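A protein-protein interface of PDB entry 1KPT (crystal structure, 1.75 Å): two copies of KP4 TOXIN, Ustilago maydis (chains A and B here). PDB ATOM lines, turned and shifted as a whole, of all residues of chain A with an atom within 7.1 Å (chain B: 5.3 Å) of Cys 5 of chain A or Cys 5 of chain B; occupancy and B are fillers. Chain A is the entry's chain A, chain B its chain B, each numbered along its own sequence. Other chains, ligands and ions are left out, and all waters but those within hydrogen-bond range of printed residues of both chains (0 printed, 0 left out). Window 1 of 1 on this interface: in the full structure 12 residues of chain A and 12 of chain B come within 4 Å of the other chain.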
ATOM      1  N   GLY A   2       6.392  -4.327  -7.379  1.00  0.00           N
ATOM      2  CA  GLY A   2       6.154  -3.385  -6.299  1.00  0.00           C
ATOM      3  C   GLY A   2       7.261  -3.555  -5.280  1.00  0.00           C
ATOM      4  O   GLY A   2       8.382  -3.928  -5.642  1.00  0.00           O
ATOM      5  N   ILE A   3       6.924  -3.358  -4.007  1.00  0.00           N
ATOM      6  CA  ILE A   3       7.885  -3.476  -2.915  1.00  0.00           C
ATOM      7  C   ILE A   3       8.589  -4.825  -2.980  1.00  0.00           C
ATOM      8  O   ILE A   3       7.951  -5.860  -3.209  1.00  0.00           O
ATOM      9  CB  ILE A   3       7.198  -3.224  -1.533  1.00  0.00           C
ATOM     10  CG1 ILE A   3       8.209  -3.343  -0.390  1.00  0.00           C
ATOM     11  CG2 ILE A   3       6.009  -4.157  -1.330  1.00  0.00           C
ATOM     12  CD1 ILE A   3       7.675  -2.821   0.920  1.00  0.00           C
ATOM     13  N   ASN A   4       9.901  -4.822  -2.801  1.00  0.00           N
ATOM     14  CA  ASN A   4      10.671  -6.062  -2.899  1.00  0.00           C
ATOM     15  C   ASN A   4      12.000  -5.952  -2.169  1.00  0.00           C
ATOM     16  O   ASN A   4      12.421  -4.858  -1.822  1.00  0.00           O
ATOM     17  CB  ASN A   4      10.888  -6.405  -4.384  1.00  0.00           C
ATOM     18  CG  ASN A   4      11.811  -5.414  -5.092  1.00  0.00           C
ATOM     19  OD1 ASN A   4      13.033  -5.496  -4.962  1.00  0.00           O
ATOM     20  ND2 ASN A   4      11.234  -4.490  -5.848  1.00  0.00           N
ATOM     21  N   CYS A   5      12.668  -7.077  -1.939  1.00  0.00           N
ATOM     22  CA  CYS A   5      13.949  -7.051  -1.241  1.00  0.00           C
ATOM     23  C   CYS A   5      15.107  -7.380  -2.180  1.00  0.00           C
ATOM     24  O   CYS A   5      16.117  -7.895  -1.745  1.00  0.00           O
ATOM     25  CB  CYS A   5      13.975  -8.040  -0.066  1.00  0.00           C
ATOM     26  SG  CYS A   5      12.653  -7.836   1.188  1.00  0.00           S
ATOM     27  N   ARG A   6      14.927  -7.139  -3.468  1.00  0.00           N
ATOM     28  CA  ARG A   6      15.975  -7.428  -4.440  1.00  0.00           C
ATOM     29  C   ARG A   6      17.177  -6.530  -4.204  1.00  0.00           C
ATOM     30  O   ARG A   6      17.029  -5.368  -3.826  1.00  0.00           O
ATOM     31  CB  ARG A   6      15.453  -7.202  -5.861  1.00  0.00           C
ATOM     32  CG  ARG A   6      14.470  -8.272  -6.342  1.00  0.00           C
ATOM     33  CD  ARG A   6      13.970  -7.956  -7.740  1.00  0.00           C
ATOM     34  NE  ARG A   6      12.832  -8.794  -8.100  1.00  0.00           N
ATOM     35  CZ  ARG A   6      12.389  -8.978  -9.344  1.00  0.00           C
ATOM     36  NH1 ARG A   6      12.993  -8.382 -10.375  1.00  0.00           N
ATOM     37  NH2 ARG A   6      11.323  -9.752  -9.555  1.00  0.00           N
ATOM     38  N   GLY A   7      18.361  -7.049  -4.481  1.00  0.00           N
ATOM     39  CA  GLY A   7      19.562  -6.262  -4.322  1.00  0.00           C
ATOM     40  C   GLY A   7      20.773  -7.060  -4.756  1.00  0.00           C
ATOM     41  O   GLY A   7      20.671  -8.226  -5.149  1.00  0.00           O
ATOM     42  N   SER A   8      21.926  -6.421  -4.704  1.00  0.00           N
ATOM     43  CA  SER A   8      23.167  -7.074  -5.060  1.00  0.00           C
ATOM     44  C   SER A   8      23.456  -8.236  -4.095  1.00  0.00           C
ATOM     45  O   SER A   8      23.069  -8.207  -2.926  1.00  0.00           O
ATOM     46  CB  SER A   8      24.291  -6.043  -4.990  1.00  0.00           C
ATOM     47  OG  SER A   8      25.558  -6.668  -4.958  1.00  0.00           O
ATOM     48  N   CYS A  11      24.564  -7.618  -0.552  1.00  0.00           N
ATOM     49  CA  CYS A  11      23.594  -7.316   0.495  1.00  0.00           C
ATOM     50  C   CYS A  11      23.543  -8.453   1.491  1.00  0.00           C
ATOM     51  O   CYS A  11      23.624  -8.234   2.702  1.00  0.00           O
ATOM     52  CB  CYS A  11      22.212  -7.132  -0.120  1.00  0.00           C
ATOM     53  SG  CYS A  11      22.109  -5.682  -1.212  1.00  0.00           S
ATOM     54  N   MET A  19      18.890  -2.358   7.278  1.00  0.00           N
ATOM     55  CA  MET A  19      17.681  -1.645   6.848  1.00  0.00           C
ATOM     56  C   MET A  19      17.102  -0.799   7.996  1.00  0.00           C
ATOM     57  O   MET A  19      16.695   0.339   7.778  1.00  0.00           O
ATOM     58  CB  MET A  19      16.613  -2.614   6.307  1.00  0.00           C
ATOM     59  CG  MET A  19      15.440  -1.926   5.620  1.00  0.00           C
ATOM     60  SD  MET A  19      15.865  -0.893   4.141  1.00  0.00           S
ATOM     61  CE  MET A  19      15.905  -2.228   2.804  1.00  0.00           C
ATOM     62  N   LEU A  73       9.890  -0.931   3.987  1.00  0.00           N
ATOM     63  CA  LEU A  73      10.887  -1.961   3.716  1.00  0.00           C
ATOM     64  C   LEU A  73      11.210  -2.783   4.953  1.00  0.00           C
ATOM     65  O   LEU A  73      11.347  -4.001   4.871  1.00  0.00           O
ATOM     66  CB  LEU A  73      12.155  -1.335   3.114  1.00  0.00           C
ATOM     67  CG  LEU A  73      11.976  -0.920   1.638  1.00  0.00           C
ATOM     68  CD1 LEU A  73      13.125  -0.037   1.139  1.00  0.00           C
ATOM     69  CD2 LEU A  73      11.887  -2.206   0.784  1.00  0.00           C
ATOM     70  N   ASN A  75       9.212  -3.295   7.513  1.00  0.00           N
ATOM     71  CA  ASN A  75       8.026  -4.104   7.789  1.00  0.00           C
ATOM     72  C   ASN A  75       7.811  -5.245   6.793  1.00  0.00           C
ATOM     73  O   ASN A  75       7.146  -6.234   7.099  1.00  0.00           O
ATOM     74  CB  ASN A  75       6.801  -3.209   7.856  1.00  0.00           C
ATOM     75  CG  ASN A  75       6.866  -2.222   9.026  1.00  0.00           C
ATOM     76  OD1 ASN A  75       7.686  -2.371   9.940  1.00  0.00           O
ATOM     77  ND2 ASN A  75       6.006  -1.209   8.996  1.00  0.00           N
ATOM     78  N   HIS A  76       8.394  -5.107   5.610  1.00  0.00           N
ATOM     79  CA  HIS A  76       8.285  -6.121   4.568  1.00  0.00           C
ATOM     80  C   HIS A  76       9.208  -7.292   4.839  1.00  0.00           C
ATOM     81  O   HIS A  76       9.070  -8.362   4.233  1.00  0.00           O
ATOM     82  CB  HIS A  76       8.626  -5.521   3.206  1.00  0.00           C
ATOM     83  CG  HIS A  76       8.030  -6.278   2.060  1.00  0.00           C
ATOM     84  ND1 HIS A  76       8.797  -6.922   1.113  1.00  0.00           N
ATOM     85  CD2 HIS A  76       6.740  -6.510   1.723  1.00  0.00           C
ATOM     86  CE1 HIS A  76       8.001  -7.522   0.241  1.00  0.00           C
ATOM     87  NE2 HIS A  76       6.752  -7.288   0.592  1.00  0.00           N
ATOM     88  N   GLY A  77      10.182  -7.086   5.714  1.00  0.00           N
ATOM     89  CA  GLY A  77      11.105  -8.159   6.031  1.00  0.00           C
ATOM     90  C   GLY A  77      12.462  -8.033   5.363  1.00  0.00           C
ATOM     91  O   GLY A  77      13.278  -8.943   5.477  1.00  0.00           O
ATOM     92  N   CYS A  78      12.705  -6.927   4.658  1.00  0.00           N
ATOM     93  CA  CYS A  78      14.006  -6.726   3.997  1.00  0.00           C
ATOM     94  C   CYS A  78      15.064  -6.343   5.029  1.00  0.00           C
ATOM     95  O   CYS A  78      15.046  -5.236   5.551  1.00  0.00           O
ATOM     96  CB  CYS A  78      13.934  -5.644   2.924  1.00  0.00           C
ATOM     97  SG  CYS A  78      12.659  -5.850   1.646  1.00  0.00           S
ATOM     98  N   ARG A  79      16.001  -7.243   5.297  1.00  0.00           N
ATOM     99  CA  ARG A  79      17.038  -6.979   6.282  1.00  0.00           C
ATOM    100  C   ARG A  79      18.124  -5.994   5.882  1.00  0.00           C
ATOM    101  O   ARG A  79      18.602  -5.249   6.735  1.00  0.00           O
ATOM    102  CB  ARG A  79      17.702  -8.277   6.732  1.00  0.00           C
ATOM    103  CG  ARG A  79      18.775  -8.076   7.817  1.00  0.00           C
ATOM    104  CD  ARG A  79      19.417  -9.399   8.258  1.00  0.00           C
ATOM    105  NE  ARG A  79      20.156 -10.071   7.190  1.00  0.00           N
ATOM    106  CZ  ARG A  79      21.430  -9.825   6.880  1.00  0.00           C
ATOM    107  NH1 ARG A  79      22.134  -8.922   7.551  1.00  0.00           N
ATOM    108  NH2 ARG A  79      21.998 -10.461   5.870  1.00  0.00           N
ATOM    109  N   VAL A  80      18.535  -6.001   4.609  1.00  0.00           N
ATOM    110  CA  VAL A  80      19.619  -5.128   4.147  1.00  0.00           C
ATOM    111  C   VAL A  80      19.320  -4.280   2.906  1.00  0.00           C
ATOM    112  O   VAL A  80      19.650  -3.093   2.871  1.00  0.00           O
ATOM    113  CB  VAL A  80      20.913  -5.951   3.849  1.00  0.00           C
ATOM    114  CG1 VAL A  80      22.078  -5.032   3.556  1.00  0.00           C
ATOM    115  CG2 VAL A  80      21.253  -6.872   4.992  1.00  0.00           C
ATOM    116  N   CYS A  81      18.703  -4.877   1.886  1.00  0.00           N
ATOM    117  CA  CYS A  81      18.416  -4.147   0.653  1.00  0.00           C
ATOM    118  C   CYS A  81      17.005  -4.413   0.201  1.00  0.00           C
ATOM    119  O   CYS A  81      16.392  -5.377   0.648  1.00  0.00           O
ATOM    120  CB  CYS A  81      19.379  -4.570  -0.465  1.00  0.00           C
ATOM    121  SG  CYS A  81      21.131  -4.317  -0.067  1.00  0.00           S
ATOM    122  N   GLY A  82      16.508  -3.561  -0.688  1.00  0.00           N
ATOM    123  CA  GLY A  82      15.157  -3.691  -1.212  1.00  0.00           C
ATOM    124  C   GLY A  82      14.694  -2.353  -1.748  1.00  0.00           C
ATOM    125  O   GLY A  82      15.377  -1.347  -1.569  1.00  0.00           O
ATOM    126  N   SER A  83      13.534  -2.312  -2.380  1.00  0.00           N
ATOM    127  CA  SER A  83      13.034  -1.070  -2.936  1.00  0.00           C
ATOM    128  C   SER A  83      11.539  -0.969  -2.720  1.00  0.00           C
ATOM    129  O   SER A  83      10.842  -1.981  -2.690  1.00  0.00           O
ATOM    130  CB  SER A  83      13.311  -1.002  -4.441  1.00  0.00           C
ATOM    131  OG  SER A  83      14.703  -1.027  -4.723  1.00  0.00           O
ATOM    132  N   VAL A  99      17.429   0.758  -1.641  1.00  0.00           N
ATOM    133  CA  VAL A  99      18.509   0.585  -0.697  1.00  0.00           C
ATOM    134  C   VAL A  99      19.315  -0.556  -1.317  1.00  0.00           C
ATOM    135  O   VAL A  99      18.811  -1.680  -1.469  1.00  0.00           O
ATOM    136  CB  VAL A  99      17.999   0.188   0.690  1.00  0.00           C
ATOM    137  CG1 VAL A  99      19.182   0.004   1.651  1.00  0.00           C
ATOM    138  CG2 VAL A  99      17.032   1.269   1.198  1.00  0.00           C
ATOM    139  N   ILE B   3       3.235 -11.580  -1.189  1.00  0.00           N
ATOM    140  CA  ILE B   3       4.589 -12.105  -1.025  1.00  0.00           C
ATOM    141  C   ILE B   3       5.406 -11.150  -0.143  1.00  0.00           C
ATOM    142  O   ILE B   3       5.325  -9.933  -0.303  1.00  0.00           O
ATOM    143  CB  ILE B   3       5.274 -12.289  -2.401  1.00  0.00           C
ATOM    144  CG1 ILE B   3       6.586 -13.042  -2.237  1.00  0.00           C
ATOM    145  CG2 ILE B   3       5.462 -10.929  -3.115  1.00  0.00           C
ATOM    146  CD1 ILE B   3       7.110 -13.638  -3.548  1.00  0.00           C
ATOM    147  N   ASN B   4       6.213 -11.692   0.760  1.00  0.00           N
ATOM    148  CA  ASN B   4       7.002 -10.853   1.672  1.00  0.00           C
ATOM    149  C   ASN B   4       8.153 -11.673   2.237  1.00  0.00           C
ATOM    150  O   ASN B   4       8.172 -12.896   2.075  1.00  0.00           O
ATOM    151  CB  ASN B   4       6.109 -10.343   2.817  1.00  0.00           C
ATOM    152  CG  ASN B   4       5.600 -11.460   3.700  1.00  0.00           C
ATOM    153  OD1 ASN B   4       6.281 -11.900   4.627  1.00  0.00           O
ATOM    154  ND2 ASN B   4       4.410 -11.952   3.395  1.00  0.00           N
ATOM    155  N   CYS B   5       9.115 -11.019   2.882  1.00  0.00           N
ATOM    156  CA  CYS B   5      10.251 -11.749   3.445  1.00  0.00           C
ATOM    157  C   CYS B   5      10.229 -11.736   4.972  1.00  0.00           C
ATOM    158  O   CYS B   5      11.275 -11.849   5.614  1.00  0.00           O
ATOM    159  CB  CYS B   5      11.598 -11.190   2.943  1.00  0.00           C
ATOM    160  SG  CYS B   5      11.753 -11.042   1.130  1.00  0.00           S
ATOM    161  N   ARG B   6       9.040 -11.616   5.562  1.00  0.00           N
ATOM    162  CA  ARG B   6       8.923 -11.606   7.024  1.00  0.00           C
ATOM    163  C   ARG B   6       9.251 -12.974   7.588  1.00  0.00           C
ATOM    164  O   ARG B   6       9.006 -13.996   6.954  1.00  0.00           O
ATOM    165  CB  ARG B   6       7.503 -11.229   7.468  1.00  0.00           C
ATOM    166  CG  ARG B   6       7.086  -9.821   7.141  1.00  0.00           C
ATOM    167  CD  ARG B   6       5.636  -9.597   7.556  1.00  0.00           C
ATOM    168  NE  ARG B   6       5.121  -8.323   7.052  1.00  0.00           N
ATOM    169  CZ  ARG B   6       3.974  -7.759   7.449  1.00  0.00           C
ATOM    170  NH1 ARG B   6       3.205  -8.343   8.368  1.00  0.00           N
ATOM    171  NH2 ARG B   6       3.572  -6.624   6.893  1.00  0.00           N
ATOM    172  N   GLY B   7       9.820 -12.993   8.782  1.00  0.00           N
ATOM    173  CA  GLY B   7      10.140 -14.255   9.408  1.00  0.00           C
ATOM    174  C   GLY B   7      10.727 -13.948  10.755  1.00  0.00           C
ATOM    175  O   GLY B   7      10.857 -12.784  11.139  1.00  0.00           O
ATOM    176  N   HIS B  76      11.992 -12.660  -5.428  1.00  0.00           N
ATOM    177  CA  HIS B  76      11.559 -11.473  -4.703  1.00  0.00           C
ATOM    178  C   HIS B  76      12.691 -10.879  -3.859  1.00  0.00           C
ATOM    179  O   HIS B  76      12.572  -9.751  -3.359  1.00  0.00           O
ATOM    180  CB  HIS B  76      10.398 -11.827  -3.778  1.00  0.00           C
ATOM    181  CG  HIS B  76       9.603 -10.640  -3.349  1.00  0.00           C
ATOM    182  ND1 HIS B  76       9.499 -10.250  -2.034  1.00  0.00           N
ATOM    183  CD2 HIS B  76       8.858  -9.765  -4.068  1.00  0.00           C
ATOM    184  CE1 HIS B  76       8.722  -9.186  -1.957  1.00  0.00           C
ATOM    185  NE2 HIS B  76       8.322  -8.869  -3.174  1.00  0.00           N
ATOM    186  N   GLY B  77      13.746 -11.662  -3.640  1.00  0.00           N
ATOM    187  CA  GLY B  77      14.874 -11.199  -2.856  1.00  0.00           C
ATOM    188  C   GLY B  77      14.964 -11.781  -1.457  1.00  0.00           C
ATOM    189  O   GLY B  77      15.880 -11.442  -0.710  1.00  0.00           O
ATOM    190  N   CYS B  78      14.036 -12.658  -1.082  1.00  0.00           N
ATOM    191  CA  CYS B  78      14.080 -13.241   0.252  1.00  0.00           C
ATOM    192  C   CYS B  78      15.205 -14.254   0.285  1.00  0.00           C
ATOM    193  O   CYS B  78      15.124 -15.306  -0.353  1.00  0.00           O
ATOM    194  CB  CYS B  78      12.750 -13.909   0.617  1.00  0.00           C
ATOM    195  SG  CYS B  78      11.274 -12.884   0.400  1.00  0.00           S
ATOM    196  N   CYS B  81      14.095 -16.285   4.745  1.00  0.00           N
ATOM    197  CA  CYS B  81      12.703 -16.515   5.132  1.00  0.00           C
ATOM    198  C   CYS B  81      11.723 -15.637   4.377  1.00  0.00           C
ATOM    199  O   CYS B  81      12.093 -14.572   3.871  1.00  0.00           O
ATOM    200  CB  CYS B  81      12.530 -16.260   6.634  1.00  0.00           C
ATOM    201  SG  CYS B  81      13.486 -17.386   7.679  1.00  0.00           S
ATOM    202  N   GLY B  82      10.469 -16.082   4.304  1.00  0.00           N
ATOM    203  CA  GLY B  82       9.441 -15.324   3.621  1.00  0.00           C
ATOM    204  C   GLY B  82       8.227 -16.198   3.356  1.00  0.00           C
ATOM    205  O   GLY B  82       8.258 -17.392   3.636  1.00  0.00           O
ATOM    206  N   SER B  83       7.168 -15.616   2.812  1.00  0.00           N
ATOM    207  CA  SER B  83       5.957 -16.370   2.500  1.00  0.00           C
ATOM    208  C   SER B  83       5.369 -15.903   1.186  1.00  0.00           C
ATOM    209  O   SER B  83       5.472 -14.731   0.832  1.00  0.00           O
ATOM    210  CB  SER B  83       4.899 -16.198   3.608  1.00  0.00           C
ATOM    211  OG  SER B  83       5.407 -16.705   4.825  1.00  0.00           O
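The backbone carbonyl oxygen of Ile 3 of chain A is in hydrogen-bond range of a ring nitrogen (NE2) of His 76 of chain B (3.0 Å). N of Cys 5 of chain A lies within hydrogen-bond range of O of His 76 of chain B (3.0 Å). NE of Arg 6 of chain B lies within hydrogen-bond range of O of Asn 75 of chain A. A ring nitrogen (NE2) of His 76 of chain A is in hydrogen-bond range of the backbone carbonyl oxygen (O) of Ile 3 of chain B (3.1 Å). The backbone carbonyl oxygen (O) of His 76 of chain A is in hydrogen-bond range of the backbone NH (N) of Cys 5 of chain B, 3.0 Å away. The side-chain sulfur of Cys 5 of chain B lies close to the side-chain sulfur of Cys 5 of chain A (3.3 Å).
The backbone carbonyl oxygen of Gly 2 of chain A is in hydrogen-bond range of the side-chain amide nitrogen of Asn 4 of chain A (2.9 Å). O of Asn 4 of chain A is in hydrogen-bond range of N of Ser 83 of chain A (2.8 Å). The side-chain sulfur of Cys 78 of chain A forms a disulfide with the side-chain sulfur of Cys 5 of chain A, 2.0 Å away. The backbone NH of Arg 6 of chain B lies within hydrogen-bond range of the side-chain amide oxygen of Asn 4 of chain B. O of Asn 4 of chain B sits at hydrogen-bond distance from N of Ser 83 of chain B, at 3.0 Å. The side-chain sulfur (SG) of Cys 81 of chain A forms a disulfide with the side-chain sulfur (SG) of Cys 11 of chain A (2.0 Å).
Among the printed residues, pairs that only touch across the chains: His 76 of chain A with His 76 of chain B, His 76 of chain A with Arg 6 of chain B, Arg 6 of chain A with His 76 of chain B, Gly 77 of chain A with Cys 5 of chain B, Asn 4 of chain A with His 76 of chain B, Cys 5 of chain A with Gly 77 of chain B and His 76 of chain A with Asn 4 of chain B.
Of the printed residues of chain B, Cys 5 of chain A touches Cys 5 (3.3 Å), His 76 (3.0 Å) and Gly 77 (3.7 Å). Met 19 of chain A touches none of the printed residues of chain B. Of the printed residues of chain B, Asn 75 of chain A touches Arg 6. Of the printed residues of chain B, His 76 of chain A touches Ile 3 (3.1 Å), Asn 4 (3.7 Å), Cys 5 (3.0 Å), Arg 6 (3.5 Å) and His 76 (2.8 Å). Cys 5 of chain B touches just these residues of chain A: Cys 5, His 76 and Gly 77. The nearest printed residue of chain A that does not touch Gly 77 of chain B is Arg 6 of chain A (4.1 Å).
Hydrophobic or aromatic side chains of chain A within 4 Å of the printed part of chain B: His 76. Of the 11 printed residues of chain B, 6 touch a printed residue of chain A. Among the printed residues, no Asp or Glu carboxylate lies within 4 Å of a Lys or Arg side-chain nitrogen of the other chain.
Asn 4 of chain A touches His 76 of chain B, and with the chains exchanged His 76 of chain A touches Asn 4 of chain B. Cys 5 of chain A touches His 76 of chain B, and with the chains exchanged His 76 of chain A touches Cys 5 of chain B. Arg 6 of chain A touches His 76 of chain B, and with the chains exchanged His 76 of chain A touches Arg 6 of chain B. His 76 of chain A touches its own counterpart, His 76 of chain B. Positions printed for both chains: 3, 4, 5, 6, 7, 76, 77, 78, 81, 82 and 83. Of the 13 pairs that touch across the chains among the printed residues, 12 have their exchanged pair printed and touching as well.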
